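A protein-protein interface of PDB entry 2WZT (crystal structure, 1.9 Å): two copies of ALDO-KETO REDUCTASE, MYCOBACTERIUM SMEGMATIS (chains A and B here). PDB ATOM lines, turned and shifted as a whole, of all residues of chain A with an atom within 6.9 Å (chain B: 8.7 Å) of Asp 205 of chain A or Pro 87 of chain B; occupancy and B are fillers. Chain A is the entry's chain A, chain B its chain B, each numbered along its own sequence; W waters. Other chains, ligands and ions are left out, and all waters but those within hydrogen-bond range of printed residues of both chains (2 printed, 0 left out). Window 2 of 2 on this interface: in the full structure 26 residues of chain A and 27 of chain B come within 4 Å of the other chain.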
ATOM      1  N   GLY A 201      22.785  -9.463  -7.522  1.00  0.00           N
ATOM      2  CA  GLY A 201      23.855 -10.182  -8.220  1.00  0.00           C
ATOM      3  C   GLY A 201      23.467 -11.044  -9.405  1.00  0.00           C
ATOM      4  O   GLY A 201      24.324 -11.387 -10.203  1.00  0.00           O
ATOM      5  N   ARG A 202      22.186 -11.412  -9.517  1.00  0.00           N
ATOM      6  CA  ARG A 202      21.737 -12.387 -10.533  1.00  0.00           C
ATOM      7  C   ARG A 202      21.873 -11.879 -11.982  1.00  0.00           C
ATOM      8  O   ARG A 202      22.131 -12.664 -12.899  1.00  0.00           O
ATOM      9  CB  ARG A 202      20.270 -12.765 -10.292  1.00  0.00           C
ATOM     10  CG  ARG A 202      20.035 -13.889  -9.296  1.00  0.00           C
ATOM     11  CD  ARG A 202      20.401 -13.529  -7.872  1.00  0.00           C
ATOM     12  NE  ARG A 202      20.096 -14.666  -7.007  1.00  0.00           N
ATOM     13  CZ  ARG A 202      20.377 -14.733  -5.717  1.00  0.00           C
ATOM     14  NH1 ARG A 202      21.011 -13.717  -5.130  1.00  0.00           N
ATOM     15  NH2 ARG A 202      20.046 -15.837  -5.035  1.00  0.00           N
ATOM     16  N   LEU A 203      21.689 -10.570 -12.172  1.00  0.00           N
ATOM     17  CA  LEU A 203      21.719  -9.973 -13.511  1.00  0.00           C
ATOM     18  C   LEU A 203      23.108 -10.039 -14.152  1.00  0.00           C
ATOM     19  O   LEU A 203      23.240  -9.929 -15.376  1.00  0.00           O
ATOM     20  CB  LEU A 203      21.210  -8.536 -13.473  1.00  0.00           C
ATOM     21  CG  LEU A 203      19.710  -8.493 -13.208  1.00  0.00           C
ATOM     22  CD1 LEU A 203      19.377  -7.134 -12.674  1.00  0.00           C
ATOM     23  CD2 LEU A 203      18.929  -8.811 -14.484  1.00  0.00           C
ATOM     24  N   LEU A 204      24.131 -10.247 -13.321  1.00  0.00           N
ATOM     25  CA  LEU A 204      25.506 -10.469 -13.794  1.00  0.00           C
ATOM     26  C   LEU A 204      25.610 -11.635 -14.776  1.00  0.00           C
ATOM     27  O   LEU A 204      26.517 -11.653 -15.595  1.00  0.00           O
ATOM     28  CB  LEU A 204      26.463 -10.669 -12.617  1.00  0.00           C
ATOM     29  CG  LEU A 204      26.681  -9.425 -11.732  1.00  0.00           C
ATOM     30  CD1 LEU A 204      27.682  -9.741 -10.605  1.00  0.00           C
ATOM     31  CD2 LEU A 204      27.123  -8.159 -12.552  1.00  0.00           C
ATOM     32  N   ASP A 205      24.683 -12.596 -14.690  1.00  0.00           N
ATOM     33  CA  ASP A 205      24.690 -13.792 -15.542  1.00  0.00           C
ATOM     34  C   ASP A 205      23.489 -13.814 -16.510  1.00  0.00           C
ATOM     35  O   ASP A 205      23.237 -14.813 -17.194  1.00  0.00           O
ATOM     36  CB  ASP A 205      24.708 -15.055 -14.651  1.00  0.00           C
ATOM     37  CG  ASP A 205      24.974 -16.335 -15.422  1.00  0.00           C
ATOM     38  OD1 ASP A 205      25.856 -16.336 -16.285  1.00  0.00           O
ATOM     39  OD2 ASP A 205      24.319 -17.359 -15.141  1.00  0.00           O
ATOM     40  N   HIS A 206      22.753 -12.712 -16.602  1.00  0.00           N
ATOM     41  CA  HIS A 206      21.600 -12.686 -17.498  1.00  0.00           C
ATOM     42  C   HIS A 206      22.110 -12.720 -18.960  1.00  0.00           C
ATOM     43  O   HIS A 206      22.989 -11.928 -19.312  1.00  0.00           O
ATOM     44  CB  HIS A 206      20.743 -11.420 -17.268  1.00  0.00           C
ATOM     45  CG  HIS A 206      19.425 -11.471 -17.979  1.00  0.00           C
ATOM     46  ND1 HIS A 206      19.316 -11.384 -19.352  1.00  0.00           N
ATOM     47  CD2 HIS A 206      18.173 -11.691 -17.514  1.00  0.00           C
ATOM     48  CE1 HIS A 206      18.050 -11.521 -19.700  1.00  0.00           C
ATOM     49  NE2 HIS A 206      17.336 -11.715 -18.606  1.00  0.00           N
ATOM     50  N   PRO A 207      21.541 -13.600 -19.811  1.00  0.00           N
ATOM     51  CA  PRO A 207      22.038 -13.819 -21.179  1.00  0.00           C
ATOM     52  C   PRO A 207      22.040 -12.571 -22.040  1.00  0.00           C
ATOM     53  O   PRO A 207      22.897 -12.403 -22.906  1.00  0.00           O
ATOM     54  CB  PRO A 207      21.048 -14.851 -21.758  1.00  0.00           C
ATOM     55  CG  PRO A 207      19.899 -14.847 -20.869  1.00  0.00           C
ATOM     56  CD  PRO A 207      20.399 -14.488 -19.512  1.00  0.00           C
ATOM     57  N   ALA A 208      21.077 -11.698 -21.814  1.00  0.00           N
ATOM     58  CA  ALA A 208      21.003 -10.479 -22.614  1.00  0.00           C
ATOM     59  C   ALA A 208      22.107  -9.502 -22.196  1.00  0.00           C
ATOM     60  O   ALA A 208      22.691  -8.846 -23.040  1.00  0.00           O
ATOM     61  CB  ALA A 208      19.610  -9.853 -22.504  1.00  0.00           C
ATOM     62  N   VAL A 209      22.362  -9.390 -20.884  1.00  0.00           N
ATOM     63  CA  VAL A 209      23.456  -8.569 -20.353  1.00  0.00           C
ATOM     64  C   VAL A 209      24.818  -9.066 -20.866  1.00  0.00           C
ATOM     65  O   VAL A 209      25.659  -8.270 -21.297  1.00  0.00           O
ATOM     66  CB  VAL A 209      23.480  -8.588 -18.799  1.00  0.00           C
ATOM     67  CG1 VAL A 209      24.684  -7.761 -18.260  1.00  0.00           C
ATOM     68  CG2 VAL A 209      22.153  -8.068 -18.230  1.00  0.00           C
ATOM     69  N   THR A 210      25.030 -10.386 -20.788  1.00  0.00           N
ATOM     70  CA  THR A 210      26.278 -10.991 -21.202  1.00  0.00           C
ATOM     71  C   THR A 210      26.532 -10.829 -22.707  1.00  0.00           C
ATOM     72  O   THR A 210      27.664 -10.538 -23.108  1.00  0.00           O
ATOM     73  CB  THR A 210      26.412 -12.496 -20.751  1.00  0.00           C
ATOM     74  OG1 THR A 210      25.555 -13.331 -21.521  1.00  0.00           O
ATOM     75  CG2 THR A 210      26.042 -12.662 -19.332  1.00  0.00           C
ATOM     76  N   ALA A 220      29.718  -7.398 -17.338  1.00  0.00           N
ATOM     77  CA  ALA A 220      28.270  -7.372 -17.132  1.00  0.00           C
ATOM     78  C   ALA A 220      27.833  -6.223 -16.215  1.00  0.00           C
ATOM     79  O   ALA A 220      26.810  -5.571 -16.480  1.00  0.00           O
ATOM     80  CB  ALA A 220      27.772  -8.759 -16.590  1.00  0.00           C
ATOM     81  N   LEU A 224      25.312  -3.071 -16.926  1.00  0.00           N
ATOM     82  CA  LEU A 224      24.128  -2.834 -16.056  1.00  0.00           C
ATOM     83  C   LEU A 224      24.081  -1.392 -15.544  1.00  0.00           C
ATOM     84  O   LEU A 224      23.007  -0.783 -15.495  1.00  0.00           O
ATOM     85  CB  LEU A 224      24.068  -3.824 -14.899  1.00  0.00           C
ATOM     86  CG  LEU A 224      23.577  -5.221 -15.296  1.00  0.00           C
ATOM     87  CD1 LEU A 224      24.024  -6.319 -14.295  1.00  0.00           C
ATOM     88  CD2 LEU A 224      22.065  -5.231 -15.524  1.00  0.00           C
ATOM     89  N   ALA B  55      26.246 -20.860  -7.224  1.00  0.00           N
ATOM     90  CA  ALA B  55      25.966 -20.862  -8.662  1.00  0.00           C
ATOM     91  C   ALA B  55      27.301 -20.957  -9.394  1.00  0.00           C
ATOM     92  O   ALA B  55      28.297 -20.399  -8.919  1.00  0.00           O
ATOM     93  CB  ALA B  55      25.217 -19.539  -9.063  1.00  0.00           C
ATOM     94  N   ALA B  56      27.336 -21.640 -10.550  1.00  0.00           N
ATOM     95  CA  ALA B  56      28.564 -21.692 -11.335  1.00  0.00           C
ATOM     96  C   ALA B  56      29.030 -20.283 -11.733  1.00  0.00           C
ATOM     97  O   ALA B  56      30.237 -19.992 -11.724  1.00  0.00           O
ATOM     98  CB  ALA B  56      28.431 -22.658 -12.549  1.00  0.00           C
ATOM     99  N   ALA B  57      28.076 -19.390 -11.982  1.00  0.00           N
ATOM    100  CA  ALA B  57      28.380 -18.019 -12.414  1.00  0.00           C
ATOM    101  C   ALA B  57      29.091 -17.181 -11.359  1.00  0.00           C
ATOM    102  O   ALA B  57      29.761 -16.224 -11.699  1.00  0.00           O
ATOM    103  CB  ALA B  57      27.114 -17.328 -12.856  1.00  0.00           C
ATOM    104  N   TYR B  58      28.905 -17.527 -10.084  1.00  0.00           N
ATOM    105  CA  TYR B  58      29.606 -16.886  -8.960  1.00  0.00           C
ATOM    106  C   TYR B  58      31.127 -17.133  -8.968  1.00  0.00           C
ATOM    107  O   TYR B  58      31.895 -16.308  -8.460  1.00  0.00           O
ATOM    108  CB  TYR B  58      29.028 -17.359  -7.613  1.00  0.00           C
ATOM    109  CG  TYR B  58      27.562 -17.029  -7.338  1.00  0.00           C
ATOM    110  CD1 TYR B  58      26.843 -16.111  -8.136  1.00  0.00           C
ATOM    111  CD2 TYR B  58      26.927 -17.571  -6.220  1.00  0.00           C
ATOM    112  CE1 TYR B  58      25.507 -15.806  -7.861  1.00  0.00           C
ATOM    113  CE2 TYR B  58      25.578 -17.275  -5.927  1.00  0.00           C
ATOM    114  CZ  TYR B  58      24.875 -16.392  -6.755  1.00  0.00           C
ATOM    115  OH  TYR B  58      23.555 -16.070  -6.450  1.00  0.00           O
ATOM    116  N   LYS B  83      23.754 -23.863  -9.741  1.00  0.00           N
ATOM    117  CA  LYS B  83      23.011 -23.377 -10.887  1.00  0.00           C
ATOM    118  C   LYS B  83      23.828 -23.484 -12.157  1.00  0.00           C
ATOM    119  O   LYS B  83      25.064 -23.323 -12.153  1.00  0.00           O
ATOM    120  CB  LYS B  83      22.522 -21.934 -10.675  1.00  0.00           C
ATOM    121  CG  LYS B  83      21.867 -21.694  -9.287  1.00  0.00           C
ATOM    122  CD  LYS B  83      21.208 -20.316  -9.185  1.00  0.00           C
ATOM    123  CE  LYS B  83      20.733 -20.122  -7.755  1.00  0.00           C
ATOM    124  NZ  LYS B  83      21.846 -19.514  -6.957  1.00  0.00           N
ATOM    125  N   LEU B  84      23.104 -23.745 -13.244  1.00  0.00           N
ATOM    126  CA  LEU B  84      23.634 -23.710 -14.585  1.00  0.00           C
ATOM    127  C   LEU B  84      24.021 -22.268 -14.941  1.00  0.00           C
ATOM    128  O   LEU B  84      23.198 -21.356 -14.817  1.00  0.00           O
ATOM    129  CB  LEU B  84      22.556 -24.225 -15.533  1.00  0.00           C
ATOM    130  CG  LEU B  84      22.874 -24.287 -17.028  1.00  0.00           C
ATOM    131  CD1 LEU B  84      24.025 -25.234 -17.271  1.00  0.00           C
ATOM    132  CD2 LEU B  84      21.630 -24.741 -17.778  1.00  0.00           C
ATOM    133  N   ALA B  85      25.272 -22.069 -15.371  1.00  0.00           N
ATOM    134  CA  ALA B  85      25.709 -20.758 -15.830  1.00  0.00           C
ATOM    135  C   ALA B  85      25.142 -20.535 -17.217  1.00  0.00           C
ATOM    136  O   ALA B  85      25.012 -21.459 -18.005  1.00  0.00           O
ATOM    137  CB  ALA B  85      27.238 -20.658 -15.835  1.00  0.00           C
ATOM    138  N   THR B  86      24.791 -19.294 -17.507  1.00  0.00           N
ATOM    139  CA  THR B  86      24.153 -18.951 -18.767  1.00  0.00           C
ATOM    140  C   THR B  86      24.941 -19.369 -20.029  1.00  0.00           C
ATOM    141  O   THR B  86      24.341 -19.848 -21.001  1.00  0.00           O
ATOM    142  CB  THR B  86      23.709 -17.453 -18.735  1.00  0.00           C
ATOM    143  OG1 THR B  86      22.527 -17.357 -17.916  1.00  0.00           O
ATOM    144  CG2 THR B  86      23.439 -16.926 -20.095  1.00  0.00           C
ATOM    145  N   PRO B  87      26.279 -19.200 -20.034  1.00  0.00           N
ATOM    146  CA  PRO B  87      27.043 -19.723 -21.178  1.00  0.00           C
ATOM    147  C   PRO B  87      26.883 -21.221 -21.472  1.00  0.00           C
ATOM    148  O   PRO B  87      27.129 -21.637 -22.608  1.00  0.00           O
ATOM    149  CB  PRO B  87      28.487 -19.441 -20.771  1.00  0.00           C
ATOM    150  CG  PRO B  87      28.366 -18.155 -19.970  1.00  0.00           C
ATOM    151  CD  PRO B  87      27.172 -18.485 -19.094  1.00  0.00           C
ATOM    152  N   ASP B  88      26.468 -21.998 -20.474  1.00  0.00           N
ATOM    153  CA  ASP B  88      26.324 -23.462 -20.601  1.00  0.00           C
ATOM    154  C   ASP B  88      24.905 -23.982 -20.896  1.00  0.00           C
ATOM    155  O   ASP B  88      24.667 -25.202 -20.884  1.00  0.00           O
ATOM    156  CB  ASP B  88      26.897 -24.167 -19.378  1.00  0.00           C
ATOM    157  CG  ASP B  88      28.368 -23.855 -19.166  1.00  0.00           C
ATOM    158  OD1 ASP B  88      29.116 -23.761 -20.148  1.00  0.00           O
ATOM    159  OD2 ASP B  88      28.779 -23.658 -18.016  1.00  0.00           O
ATOM    160  N   GLN B  89      23.988 -23.068 -21.203  1.00  0.00           N
ATOM    161  CA  GLN B  89      22.599 -23.438 -21.502  1.00  0.00           C
ATOM    162  C   GLN B  89      22.554 -24.354 -22.718  1.00  0.00           C
ATOM    163  O   GLN B  89      23.366 -24.195 -23.664  1.00  0.00           O
ATOM    164  CB  GLN B  89      21.730 -22.204 -21.770  1.00  0.00           C
ATOM    165  CG  GLN B  89      21.274 -21.461 -20.528  1.00  0.00           C
ATOM    166  CD  GLN B  89      19.771 -21.240 -20.529  1.00  0.00           C
ATOM    167  OE1 GLN B  89      19.013 -22.156 -20.249  1.00  0.00           O
ATOM    168  NE2 GLN B  89      19.337 -20.025 -20.850  1.00  0.00           N
ATOM    169  N   GLY B  90      21.639 -25.318 -22.670  1.00  0.00           N
ATOM    170  CA  GLY B  90      21.408 -26.250 -23.786  1.00  0.00           C
ATOM    171  C   GLY B  90      21.170 -27.638 -23.211  1.00  0.00           C
ATOM    172  O   GLY B  90      21.380 -27.865 -22.028  1.00  0.00           O
ATOM    173  N   SER B  93      24.830 -29.567 -23.226  1.00  0.00           N
ATOM    174  CA  SER B  93      25.809 -28.751 -22.481  1.00  0.00           C
ATOM    175  C   SER B  93      25.457 -28.654 -20.999  1.00  0.00           C
ATOM    176  O   SER B  93      26.366 -28.655 -20.156  1.00  0.00           O
ATOM    177  CB  SER B  93      25.880 -27.340 -23.064  1.00  0.00           C
ATOM    178  OG  SER B  93      24.599 -26.741 -23.033  1.00  0.00           O
ATOM    179  N   SER B  94      24.158 -28.573 -20.674  1.00  0.00           N
ATOM    180  CA  SER B  94      23.731 -28.488 -19.253  1.00  0.00           C
ATOM    181  C   SER B  94      24.134 -29.744 -18.462  1.00  0.00           C
ATOM    182  O   SER B  94      24.457 -29.646 -17.280  1.00  0.00           O
ATOM    183  CB  SER B  94      22.209 -28.282 -19.084  1.00  0.00           C
ATOM    184  OG  SER B  94      21.483 -29.383 -19.633  1.00  0.00           O
ATOM    185  N   ALA B  97      27.733 -29.425 -17.720  1.00  0.00           N
ATOM    186  CA  ALA B  97      27.893 -28.305 -16.786  1.00  0.00           C
ATOM    187  C   ALA B  97      27.610 -28.722 -15.337  1.00  0.00           C
ATOM    188  O   ALA B  97      28.348 -28.333 -14.438  1.00  0.00           O
ATOM    189  CB  ALA B  97      26.969 -27.170 -17.185  1.00  0.00           C
ATOM    190  N   LEU B 114      19.640 -25.650 -10.510  1.00  0.00           N
ATOM    191  CA  LEU B 114      18.695 -24.675 -11.102  1.00  0.00           C
ATOM    192  C   LEU B 114      19.185 -24.105 -12.450  1.00  0.00           C
ATOM    193  O   LEU B 114      20.354 -23.791 -12.609  1.00  0.00           O
ATOM    194  CB  LEU B 114      18.453 -23.525 -10.095  1.00  0.00           C
ATOM    195  CG  LEU B 114      18.026 -23.891  -8.649  1.00  0.00           C
ATOM    196  CD1 LEU B 114      17.894 -22.632  -7.861  1.00  0.00           C
ATOM    197  CD2 LEU B 114      16.679 -24.656  -8.608  1.00  0.00           C
ATOM    198  N   ILE B 115      18.274 -23.913 -13.391  1.00  0.00           N
ATOM    199  CA  ILE B 115      18.507 -22.966 -14.491  1.00  0.00           C
ATOM    200  C   ILE B 115      18.520 -21.575 -13.868  1.00  0.00           C
ATOM    201  O   ILE B 115      17.625 -21.234 -13.085  1.00  0.00           O
ATOM    202  CB  ILE B 115      17.379 -23.046 -15.573  1.00  0.00           C
ATOM    203  CG1 ILE B 115      17.391 -24.430 -16.241  1.00  0.00           C
ATOM    204  CG2 ILE B 115      17.523 -21.932 -16.645  1.00  0.00           C
ATOM    205  CD1 ILE B 115      16.281 -24.669 -17.266  1.00  0.00           C
ATOM    206  N   HIS B 116      19.511 -20.764 -14.234  1.00  0.00           N
ATOM    207  CA  HIS B 116      19.710 -19.461 -13.597  1.00  0.00           C
ATOM    208  C   HIS B 116      18.766 -18.401 -14.196  1.00  0.00           C
ATOM    209  O   HIS B 116      18.251 -17.528 -13.477  1.00  0.00           O
ATOM    210  CB  HIS B 116      21.190 -19.047 -13.706  1.00  0.00           C
ATOM    211  CG  HIS B 116      21.632 -18.035 -12.688  1.00  0.00           C
ATOM    212  ND1 HIS B 116      22.774 -17.282 -12.847  1.00  0.00           N
ATOM    213  CD2 HIS B 116      21.091 -17.653 -11.502  1.00  0.00           C
ATOM    214  CE1 HIS B 116      22.936 -16.500 -11.791  1.00  0.00           C
ATOM    215  NE2 HIS B 116      21.920 -16.697 -10.968  1.00  0.00           N
ATOM    216  N   TRP B 117      18.536 -18.483 -15.508  1.00  0.00           N
ATOM    217  CA  TRP B 117      17.653 -17.530 -16.209  1.00  0.00           C
ATOM    218  C   TRP B 117      17.002 -18.206 -17.391  1.00  0.00           C
ATOM    219  O   TRP B 117      17.685 -18.946 -18.115  1.00  0.00           O
ATOM    220  CB  TRP B 117      18.491 -16.383 -16.806  1.00  0.00           C
ATOM    221  CG  TRP B 117      18.987 -15.434 -15.829  1.00  0.00           C
ATOM    222  CD1 TRP B 117      20.246 -15.358 -15.317  1.00  0.00           C
ATOM    223  CD2 TRP B 117      18.233 -14.377 -15.228  1.00  0.00           C
ATOM    224  NE1 TRP B 117      20.329 -14.305 -14.428  1.00  0.00           N
ATOM    225  CE2 TRP B 117      19.104 -13.691 -14.351  1.00  0.00           C
ATOM    226  CE3 TRP B 117      16.895 -13.947 -15.340  1.00  0.00           C
ATOM    227  CZ2 TRP B 117      18.687 -12.569 -13.586  1.00  0.00           C
ATOM    228  CZ3 TRP B 117      16.481 -12.838 -14.578  1.00  0.00           C
ATOM    229  CH2 TRP B 117      17.381 -12.161 -13.719  1.00  0.00           C
ATOM    230  N   PRO B 118      15.715 -17.902 -17.656  1.00  0.00           N
ATOM    231  CA  PRO B 118      15.185 -18.439 -18.913  1.00  0.00           C
ATOM    232  C   PRO B 118      15.803 -17.812 -20.178  1.00  0.00           C
ATOM    233  O   PRO B 118      16.174 -18.549 -21.099  1.00  0.00           O
ATOM    234  CB  PRO B 118      13.665 -18.195 -18.800  1.00  0.00           C
ATOM    235  CG  PRO B 118      13.536 -17.013 -17.893  1.00  0.00           C
ATOM    236  CD  PRO B 118      14.710 -17.098 -16.919  1.00  0.00           C
ATOM    237  N   GLY B 119      15.942 -16.494 -20.224  1.00  0.00           N
ATOM    238  CA  GLY B 119      16.302 -15.844 -21.480  1.00  0.00           C
ATOM    239  C   GLY B 119      15.145 -15.763 -22.484  1.00  0.00           C
ATOM    240  O   GLY B 119      14.113 -16.435 -22.331  1.00  0.00           O
ATOM    241  N   LYS B 124      16.396 -22.528 -26.106  1.00  0.00           N
ATOM    242  CA  LYS B 124      17.526 -22.754 -25.169  1.00  0.00           C
ATOM    243  C   LYS B 124      17.135 -23.196 -23.765  1.00  0.00           C
ATOM    244  O   LYS B 124      17.766 -24.088 -23.208  1.00  0.00           O
ATOM    245  CB  LYS B 124      18.435 -21.515 -25.051  1.00  0.00           C
ATOM    246  CG  LYS B 124      19.199 -21.228 -26.333  1.00  0.00           C
ATOM    247  CD  LYS B 124      20.050 -19.958 -26.252  1.00  0.00           C
ATOM    248  CE  LYS B 124      21.310 -20.178 -25.449  1.00  0.00           C
ATOM    249  NZ  LYS B 124      22.179 -21.166 -26.094  1.00  0.00           N
ATOM    250  N   SER B 128      17.655 -26.720 -22.004  1.00  0.00           N
ATOM    251  CA  SER B 128      18.289 -26.754 -20.676  1.00  0.00           C
ATOM    252  C   SER B 128      17.471 -27.595 -19.687  1.00  0.00           C
ATOM    253  O   SER B 128      18.051 -28.374 -18.948  1.00  0.00           O
ATOM    254  CB  SER B 128      18.495 -25.352 -20.105  1.00  0.00           C
ATOM    255  OG  SER B 128      19.579 -24.723 -20.760  1.00  0.00           O
HETATM  256  O   HOH W   1      22.121 -17.143  -8.336  1.00  0.00           O
HETATM  257  O   HOH W   2      14.800 -13.772 -18.622  1.00  0.00           O
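The side-chain hydroxyl of Thr 86 of chain B lies within hydrogen-bond range of the backbone carbonyl oxygen of Asp 205 of chain A (2.7 Å).
NE1 of Trp 117 of chain B sits at hydrogen-bond distance from O of Arg 202 of chain A.
OD2 of Asp 205 of chain A is in hydrogen-bond range of ND1 of His 116 of chain B (2.8 Å).
Asp 205 of chain A touches six residues of chain B.
Of the printed residues of chain A, Ala 57 of chain B touches Asp 205 (3.5 Å).
Pro 87 of chain B touches just one residue of chain A: Asp 205.
Of the printed residues of chain A, His 116 of chain B touches Arg 202 (3.8 Å) and Asp 205 (2.8 Å).
Of the printed residues of chain A, Trp 117 of chain B touches Arg 202, Leu 203, Asp 205, His 206 and Pro 207.
The nearest residue of chain A that does not touch Pro 87 of chain B is Thr 210 of chain A (5.8 Å).
O of Trp 117 of chain B sits at hydrogen-bond distance from NE2 of Gln 89 of chain B (3.4 Å).
The backbone carbonyl oxygen (O) of Pro 207 of chain A is in hydrogen-bond range of the side-chain hydroxyl (OG1) of Thr 210 of chain A (3.1 Å).
A ring nitrogen (ND1) of His 206 of chain A lies within hydrogen-bond range of the backbone NH (N) of Ala 208 of chain A.
Water W1 lies within hydrogen-bond range of the side-chain hydroxyl of Tyr 58 of chain B (2.6 Å), a ring nitrogen (NE2) of His 116 of chain B (2.7 Å), the side-chain amino group of Lys 83 of chain B (2.8 Å) and the guanidinium group of Arg 202 of chain A (3.5 Å).
Water W2 bridges a ring nitrogen (NE2) of His 206 of chain A and the backbone NH (N) of Gly 119 of chain B.
OH of Tyr 58 of chain B touches CZ of Arg 202 of chain A, 3.5 Å away.
CG of Arg 202 of chain A touches NE2 of His 116 of chain B (3.8 Å).
Trp 117 of chain B touches Leu 203 of chain A.
CG of Asp 205 of chain A touches CB of Ala 57 of chain B, at 3.5 Å.
OD2 of Asp 205 of chain A touches CA of Ala 85 of chain B, 3.7 Å away.
Asp 205 of chain A touches Pro 87 of chain B.
O of Asp 205 of chain A touches CD1 of Trp 117 of chain B, 3.6 Å away.
CE3 of Trp 117 of chain B touches CD2 of His 206 of chain A, 3.4 Å away.
CB of Pro 207 of chain A touches CG2 of Thr 86 of chain B (3.6 Å).
Trp 117 of chain B touches Pro 207 of chain A.
Of the 23 printed residues of chain B, 8 touch a printed residue of chain A.
Hydrophobic or aromatic side chains of chain B that line the printed part of chain A: Ala 57, Tyr 58, Pro 87, His 116 and Trp 117.
Printed residues of chain A that touch a printed residue of chain B: Arg 202, Leu 203, Asp 205, His 206 and Pro 207.
Among the printed residues, 14 pairs touch across the chains.
Among the printed residues, no Asp or Glu carboxylate lies within 4 Å of a Lys or Arg side-chain nitrogen of the other chain.
No position is printed for both chains.
Of the 14 pairs that touch across the chains among the printed residues, none has its exchanged pair printed and touching as well.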
